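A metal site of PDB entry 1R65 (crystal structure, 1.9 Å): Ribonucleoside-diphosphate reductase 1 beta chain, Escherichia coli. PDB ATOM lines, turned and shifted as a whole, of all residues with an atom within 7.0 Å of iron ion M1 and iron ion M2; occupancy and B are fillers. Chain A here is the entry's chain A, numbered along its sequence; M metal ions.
Iron ion M2 is bound by OE1 of Glu 238 (1.8 Å), OE2 of Glu 115 (2.1 Å) and ND1 of His 241 (2.2 Å). Slightly farther from iron ion M2 lies the side-chain carboxylate (OE1) of Glu 204 (2.6 Å). Slightly farther from iron ion M2 lies OE2 of Glu 204 (2.7 Å). Slightly farther from iron ion M2 lies the side-chain carboxylate (OE2) of Glu 238 (2.8 Å).
The side-chain carboxylate (OD2) of Asp 84 is in hydrogen-bond range of the side-chain hydroxyl (OH) of Tyr 122 (2.6 Å). A ring nitrogen (NE2) of His 118 is in hydrogen-bond range of the side-chain carboxylate (OD2) of Asp 237 (2.6 Å). O of Glu 115 lies within hydrogen-bond range of OG of Ser 119 (3.4 Å). NE1 of Trp 111 sits close to ND1 of His 241, 3.3 Å away. NE2 of His 241 is in hydrogen-bond range of OG of Ser 114 (2.9 Å). The backbone carbonyl oxygen of Asp 237 lies close to a ring nitrogen (NE2) of His 241, at 3.4 Å. The side-chain carboxylate of Glu 204 lies within hydrogen-bond range of the indole nitrogen of Trp 111 (3.1 Å). NE2 of Gln 87 sits at hydrogen-bond distance from OE2 of Glu 204 (3.3 Å).
CZ of Phe 208 touches iron ion M1 (3.7 Å). Of the 21 residues printed, 5 come within 4 Å of iron ion M1. Along chain A the residues within 4 Å of iron ion M1 span positions 84 to 238.
Iron ion M1 is bound by OD1 of Asp 84, ND1 of His 118, OE1 of Glu 115 and OE2 of Glu 238.
Trp 111 touches iron ion M2. Five residues have an atom within 4 Å of iron ion M2: Trp 111, Glu 115, Glu 204, Glu 238 and His 241. The nearest printed residue that does not touch iron ion M2 is Phe 208 (4.1 Å).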
ATOM      1  N   GLN A  80       2.021   6.694   6.399  1.00  0.00           N
ATOM      2  CA  GLN A  80       2.311   6.429   7.813  1.00  0.00           C
ATOM      3  C   GLN A  80       2.557   7.760   8.535  1.00  0.00           C
ATOM      4  O   GLN A  80       2.082   7.966   9.650  1.00  0.00           O
ATOM      5  CB  GLN A  80       3.567   5.517   7.936  1.00  0.00           C
ATOM      6  CG  GLN A  80       3.411   4.144   7.246  1.00  0.00           C
ATOM      7  CD  GLN A  80       4.689   3.292   7.274  1.00  0.00           C
ATOM      8  OE1 GLN A  80       5.778   3.783   7.001  1.00  0.00           O
ATOM      9  NE2 GLN A  80       4.531   2.018   7.600  1.00  0.00           N
ATOM     10  N   LEU A  83      -0.864   9.306   9.232  1.00  0.00           N
ATOM     11  CA  LEU A  83      -1.589   8.661  10.303  1.00  0.00           C
ATOM     12  C   LEU A  83      -1.046   9.036  11.679  1.00  0.00           C
ATOM     13  O   LEU A  83      -1.818   9.341  12.587  1.00  0.00           O
ATOM     14  CB  LEU A  83      -1.566   7.140  10.138  1.00  0.00           C
ATOM     15  CG  LEU A  83      -2.326   6.548   8.944  1.00  0.00           C
ATOM     16  CD1 LEU A  83      -2.166   5.033   8.962  1.00  0.00           C
ATOM     17  CD2 LEU A  83      -3.795   6.926   9.016  1.00  0.00           C
ATOM     18  N   ASP A  84       0.270   9.037  11.835  1.00  0.00           N
ATOM     19  CA  ASP A  84       0.846   9.394  13.122  1.00  0.00           C
ATOM     20  C   ASP A  84       0.776  10.883  13.427  1.00  0.00           C
ATOM     21  O   ASP A  84       0.785  11.278  14.598  1.00  0.00           O
ATOM     22  CB  ASP A  84       2.271   8.847  13.246  1.00  0.00           C
ATOM     23  CG  ASP A  84       2.292   7.387  13.687  1.00  0.00           C
ATOM     24  OD1 ASP A  84       1.611   7.094  14.691  1.00  0.00           O
ATOM     25  OD2 ASP A  84       2.957   6.539  13.059  1.00  0.00           O
ATOM     26  N   GLN A  87      -2.636  11.022  14.835  1.00  0.00           N
ATOM     27  CA  GLN A  87      -2.700  10.283  16.093  1.00  0.00           C
ATOM     28  C   GLN A  87      -1.856  10.872  17.219  1.00  0.00           C
ATOM     29  O   GLN A  87      -1.982  10.463  18.365  1.00  0.00           O
ATOM     30  CB  GLN A  87      -2.304   8.827  15.869  1.00  0.00           C
ATOM     31  CG  GLN A  87      -3.337   7.997  15.100  1.00  0.00           C
ATOM     32  CD  GLN A  87      -4.707   8.000  15.772  1.00  0.00           C
ATOM     33  OE1 GLN A  87      -5.547   8.869  15.502  1.00  0.00           O
ATOM     34  NE2 GLN A  87      -4.940   7.035  16.649  1.00  0.00           N
ATOM     35  N   TRP A 111      -0.338   7.134  25.014  1.00  0.00           N
ATOM     36  CA  TRP A 111      -0.566   6.618  23.681  1.00  0.00           C
ATOM     37  C   TRP A 111      -0.250   7.725  22.657  1.00  0.00           C
ATOM     38  O   TRP A 111       0.507   7.499  21.700  1.00  0.00           O
ATOM     39  CB  TRP A 111      -2.033   6.132  23.614  1.00  0.00           C
ATOM     40  CG  TRP A 111      -2.647   5.865  22.290  1.00  0.00           C
ATOM     41  CD1 TRP A 111      -2.008   5.578  21.116  1.00  0.00           C
ATOM     42  CD2 TRP A 111      -4.045   5.797  22.012  1.00  0.00           C
ATOM     43  NE1 TRP A 111      -2.932   5.318  20.136  1.00  0.00           N
ATOM     44  CE2 TRP A 111      -4.190   5.444  20.650  1.00  0.00           C
ATOM     45  CE3 TRP A 111      -5.199   5.983  22.787  1.00  0.00           C
ATOM     46  CZ2 TRP A 111      -5.442   5.283  20.048  1.00  0.00           C
ATOM     47  CZ3 TRP A 111      -6.451   5.822  22.185  1.00  0.00           C
ATOM     48  CH2 TRP A 111      -6.556   5.474  20.831  1.00  0.00           C
ATOM     49  N   SER A 114       3.495   8.423  22.444  1.00  0.00           N
ATOM     50  CA  SER A 114       4.224   7.431  21.661  1.00  0.00           C
ATOM     51  C   SER A 114       4.059   7.706  20.165  1.00  0.00           C
ATOM     52  O   SER A 114       4.947   7.394  19.378  1.00  0.00           O
ATOM     53  CB  SER A 114       3.758   6.005  21.997  1.00  0.00           C
ATOM     54  OG  SER A 114       2.486   5.714  21.437  1.00  0.00           O
ATOM     55  N   GLU A 115       2.940   8.294  19.769  1.00  0.00           N
ATOM     56  CA  GLU A 115       2.743   8.599  18.353  1.00  0.00           C
ATOM     57  C   GLU A 115       3.674   9.728  17.918  1.00  0.00           C
ATOM     58  O   GLU A 115       4.106   9.767  16.756  1.00  0.00           O
ATOM     59  CB  GLU A 115       1.278   8.962  18.056  1.00  0.00           C
ATOM     60  CG  GLU A 115       0.243   7.895  18.484  1.00  0.00           C
ATOM     61  CD  GLU A 115       0.318   6.601  17.677  1.00  0.00           C
ATOM     62  OE1 GLU A 115       1.425   6.108  17.421  1.00  0.00           O
ATOM     63  OE2 GLU A 115      -0.738   6.054  17.316  1.00  0.00           O
ATOM     64  N   THR A 116       4.003  10.656  18.820  1.00  0.00           N
ATOM     65  CA  THR A 116       4.909  11.751  18.432  1.00  0.00           C
ATOM     66  C   THR A 116       6.309  11.185  18.213  1.00  0.00           C
ATOM     67  O   THR A 116       7.063  11.700  17.400  1.00  0.00           O
ATOM     68  CB  THR A 116       4.990  12.891  19.484  1.00  0.00           C
ATOM     69  OG1 THR A 116       5.529  12.386  20.723  1.00  0.00           O
ATOM     70  CG2 THR A 116       3.614  13.486  19.706  1.00  0.00           C
ATOM     71  N   HIS A 118       6.813   8.303  16.939  1.00  0.00           N
ATOM     72  CA  HIS A 118       6.705   7.689  15.626  1.00  0.00           C
ATOM     73  C   HIS A 118       6.907   8.758  14.560  1.00  0.00           C
ATOM     74  O   HIS A 118       7.608   8.547  13.563  1.00  0.00           O
ATOM     75  CB  HIS A 118       5.346   7.014  15.464  1.00  0.00           C
ATOM     76  CG  HIS A 118       5.137   5.870  16.413  1.00  0.00           C
ATOM     77  ND1 HIS A 118       3.939   5.198  16.523  1.00  0.00           N
ATOM     78  CD2 HIS A 118       5.980   5.291  17.304  1.00  0.00           C
ATOM     79  CE1 HIS A 118       4.051   4.259  17.438  1.00  0.00           C
ATOM     80  NE2 HIS A 118       5.272   4.293  17.936  1.00  0.00           N
ATOM     81  N   SER A 119       6.303   9.927  14.755  1.00  0.00           N
ATOM     82  CA  SER A 119       6.459  11.034  13.803  1.00  0.00           C
ATOM     83  C   SER A 119       7.920  11.442  13.738  1.00  0.00           C
ATOM     84  O   SER A 119       8.453  11.716  12.659  1.00  0.00           O
ATOM     85  CB  SER A 119       5.602  12.227  14.220  1.00  0.00           C
ATOM     86  OG  SER A 119       4.230  11.914  14.124  1.00  0.00           O
ATOM     87  N   TYR A 122       9.868   9.116  11.466  1.00  0.00           N
ATOM     88  CA  TYR A 122       9.683   9.302  10.026  1.00  0.00           C
ATOM     89  C   TYR A 122      10.559  10.441   9.522  1.00  0.00           C
ATOM     90  O   TYR A 122      11.048  10.402   8.389  1.00  0.00           O
ATOM     91  CB  TYR A 122       8.226   9.584   9.662  1.00  0.00           C
ATOM     92  CG  TYR A 122       7.278   8.493  10.098  1.00  0.00           C
ATOM     93  CD1 TYR A 122       7.593   7.144   9.890  1.00  0.00           C
ATOM     94  CD2 TYR A 122       6.078   8.783  10.740  1.00  0.00           C
ATOM     95  CE1 TYR A 122       6.743   6.122  10.327  1.00  0.00           C
ATOM     96  CE2 TYR A 122       5.217   7.777  11.174  1.00  0.00           C
ATOM     97  CZ  TYR A 122       5.561   6.460  10.962  1.00  0.00           C
ATOM     98  OH  TYR A 122       4.717   5.456  11.410  1.00  0.00           O
ATOM     99  N   LEU A 203      -8.273   2.102  12.348  1.00  0.00           N
ATOM    100  CA  LEU A 203      -7.061   2.778  11.937  1.00  0.00           C
ATOM    101  C   LEU A 203      -5.852   2.012  12.501  1.00  0.00           C
ATOM    102  O   LEU A 203      -4.893   1.702  11.788  1.00  0.00           O
ATOM    103  CB  LEU A 203      -7.071   4.224  12.451  1.00  0.00           C
ATOM    104  CG  LEU A 203      -5.891   5.139  12.124  1.00  0.00           C
ATOM    105  CD1 LEU A 203      -6.273   6.582  12.422  1.00  0.00           C
ATOM    106  CD2 LEU A 203      -4.674   4.734  12.933  1.00  0.00           C
ATOM    107  N   GLU A 204      -5.927   1.715  13.789  1.00  0.00           N
ATOM    108  CA  GLU A 204      -4.869   1.007  14.495  1.00  0.00           C
ATOM    109  C   GLU A 204      -4.706  -0.443  14.053  1.00  0.00           C
ATOM    110  O   GLU A 204      -3.590  -0.920  13.852  1.00  0.00           O
ATOM    111  CB  GLU A 204      -5.153   1.023  16.006  1.00  0.00           C
ATOM    112  CG  GLU A 204      -5.169   2.403  16.652  1.00  0.00           C
ATOM    113  CD  GLU A 204      -3.778   2.950  16.870  1.00  0.00           C
ATOM    114  OE1 GLU A 204      -2.808   2.239  16.563  1.00  0.00           O
ATOM    115  OE2 GLU A 204      -3.655   4.101  17.349  1.00  0.00           O
ATOM    116  N   PHE A 208      -2.694   0.656   9.744  1.00  0.00           N
ATOM    117  CA  PHE A 208      -1.270   0.543  10.080  1.00  0.00           C
ATOM    118  C   PHE A 208      -0.632  -0.771   9.637  1.00  0.00           C
ATOM    119  O   PHE A 208       0.488  -0.771   9.126  1.00  0.00           O
ATOM    120  CB  PHE A 208      -1.045   0.730  11.579  1.00  0.00           C
ATOM    121  CG  PHE A 208      -0.773   2.145  11.988  1.00  0.00           C
ATOM    122  CD1 PHE A 208       0.322   2.841  11.462  1.00  0.00           C
ATOM    123  CD2 PHE A 208      -1.601   2.806  12.896  1.00  0.00           C
ATOM    124  CE1 PHE A 208       0.583   4.155  11.836  1.00  0.00           C
ATOM    125  CE2 PHE A 208      -1.346   4.118  13.277  1.00  0.00           C
ATOM    126  CZ  PHE A 208      -0.245   4.803  12.739  1.00  0.00           C
ATOM    127  N   PHE A 212       2.547  -1.763   7.233  1.00  0.00           N
ATOM    128  CA  PHE A 212       3.701  -2.505   7.733  1.00  0.00           C
ATOM    129  C   PHE A 212       4.146  -3.521   6.691  1.00  0.00           C
ATOM    130  O   PHE A 212       5.340  -3.703   6.455  1.00  0.00           O
ATOM    131  CB  PHE A 212       3.387  -3.251   9.037  1.00  0.00           C
ATOM    132  CG  PHE A 212       3.058  -2.343  10.187  1.00  0.00           C
ATOM    133  CD1 PHE A 212       3.474  -1.024  10.201  1.00  0.00           C
ATOM    134  CD2 PHE A 212       2.333  -2.836  11.277  1.00  0.00           C
ATOM    135  CE1 PHE A 212       3.177  -0.194  11.278  1.00  0.00           C
ATOM    136  CE2 PHE A 212       2.035  -2.018  12.363  1.00  0.00           C
ATOM    137  CZ  PHE A 212       2.463  -0.692  12.363  1.00  0.00           C
ATOM    138  N   ILE A 234       7.724   0.513  15.910  1.00  0.00           N
ATOM    139  CA  ILE A 234       6.451   1.186  15.759  1.00  0.00           C
ATOM    140  C   ILE A 234       5.322   0.157  15.812  1.00  0.00           C
ATOM    141  O   ILE A 234       4.317   0.381  16.494  1.00  0.00           O
ATOM    142  CB  ILE A 234       6.367   1.969  14.425  1.00  0.00           C
ATOM    143  CG1 ILE A 234       7.277   3.190  14.511  1.00  0.00           C
ATOM    144  CG2 ILE A 234       4.925   2.387  14.141  1.00  0.00           C
ATOM    145  CD1 ILE A 234       7.237   4.067  13.250  1.00  0.00           C
ATOM    146  N   ASP A 237       4.436  -0.861  19.226  1.00  0.00           N
ATOM    147  CA  ASP A 237       3.595   0.124  19.926  1.00  0.00           C
ATOM    148  C   ASP A 237       2.141   0.057  19.466  1.00  0.00           C
ATOM    149  O   ASP A 237       1.205   0.118  20.276  1.00  0.00           O
ATOM    150  CB  ASP A 237       4.115   1.557  19.691  1.00  0.00           C
ATOM    151  CG  ASP A 237       5.463   1.822  20.359  1.00  0.00           C
ATOM    152  OD1 ASP A 237       5.791   1.165  21.377  1.00  0.00           O
ATOM    153  OD2 ASP A 237       6.169   2.736  19.883  1.00  0.00           O
ATOM    154  N   GLU A 238       1.938  -0.043  18.155  1.00  0.00           N
ATOM    155  CA  GLU A 238       0.586  -0.104  17.606  1.00  0.00           C
ATOM    156  C   GLU A 238      -0.195  -1.305  18.152  1.00  0.00           C
ATOM    157  O   GLU A 238      -1.393  -1.220  18.345  1.00  0.00           O
ATOM    158  CB  GLU A 238       0.611  -0.170  16.078  1.00  0.00           C
ATOM    159  CG  GLU A 238       1.144   1.076  15.385  1.00  0.00           C
ATOM    160  CD  GLU A 238       0.698   2.360  16.070  1.00  0.00           C
ATOM    161  OE1 GLU A 238      -0.495   2.474  16.403  1.00  0.00           O
ATOM    162  OE2 GLU A 238       1.526   3.260  16.261  1.00  0.00           O
ATOM    163  N   ALA A 239       0.496  -2.409  18.380  1.00  0.00           N
ATOM    164  CA  ALA A 239      -0.163  -3.601  18.908  1.00  0.00           C
ATOM    165  C   ALA A 239      -0.736  -3.290  20.297  1.00  0.00           C
ATOM    166  O   ALA A 239      -1.794  -3.804  20.668  1.00  0.00           O
ATOM    167  CB  ALA A 239       0.828  -4.755  19.000  1.00  0.00           C
ATOM    168  N   HIS A 241      -1.625  -0.202  21.265  1.00  0.00           N
ATOM    169  CA  HIS A 241      -2.684   0.749  21.009  1.00  0.00           C
ATOM    170  C   HIS A 241      -3.964   0.046  20.590  1.00  0.00           C
ATOM    171  O   HIS A 241      -5.041   0.381  21.080  1.00  0.00           O
ATOM    172  CB  HIS A 241      -2.245   1.746  19.921  1.00  0.00           C
ATOM    173  CG  HIS A 241      -1.003   2.494  20.260  1.00  0.00           C
ATOM    174  ND1 HIS A 241      -0.377   3.352  19.381  1.00  0.00           N
ATOM    175  CD2 HIS A 241      -0.248   2.517  21.398  1.00  0.00           C
ATOM    176  CE1 HIS A 241       0.693   3.873  19.947  1.00  0.00           C
ATOM    177  NE2 HIS A 241       0.794   3.378  21.167  1.00  0.00           N
ATOM    178  N   LEU A 242      -3.854  -0.921  19.684  1.00  0.00           N
ATOM    179  CA  LEU A 242      -5.057  -1.612  19.238  1.00  0.00           C
ATOM    180  C   LEU A 242      -5.635  -2.465  20.362  1.00  0.00           C
ATOM    181  O   LEU A 242      -6.848  -2.668  20.456  1.00  0.00           O
ATOM    182  CB  LEU A 242      -4.776  -2.459  17.992  1.00  0.00           C
ATOM    183  CG  LEU A 242      -4.339  -3.923  18.043  1.00  0.00           C
ATOM    184  CD1 LEU A 242      -5.460  -4.778  18.607  1.00  0.00           C
ATOM    185  CD2 LEU A 242      -4.015  -4.387  16.631  1.00  0.00           C
HETATM  186 FE    FE M   1       2.069   5.301  15.553  1.00  0.00          FE
HETATM  187 FE    FE M   2      -0.992   3.958  17.370  1.00  0.00          FE
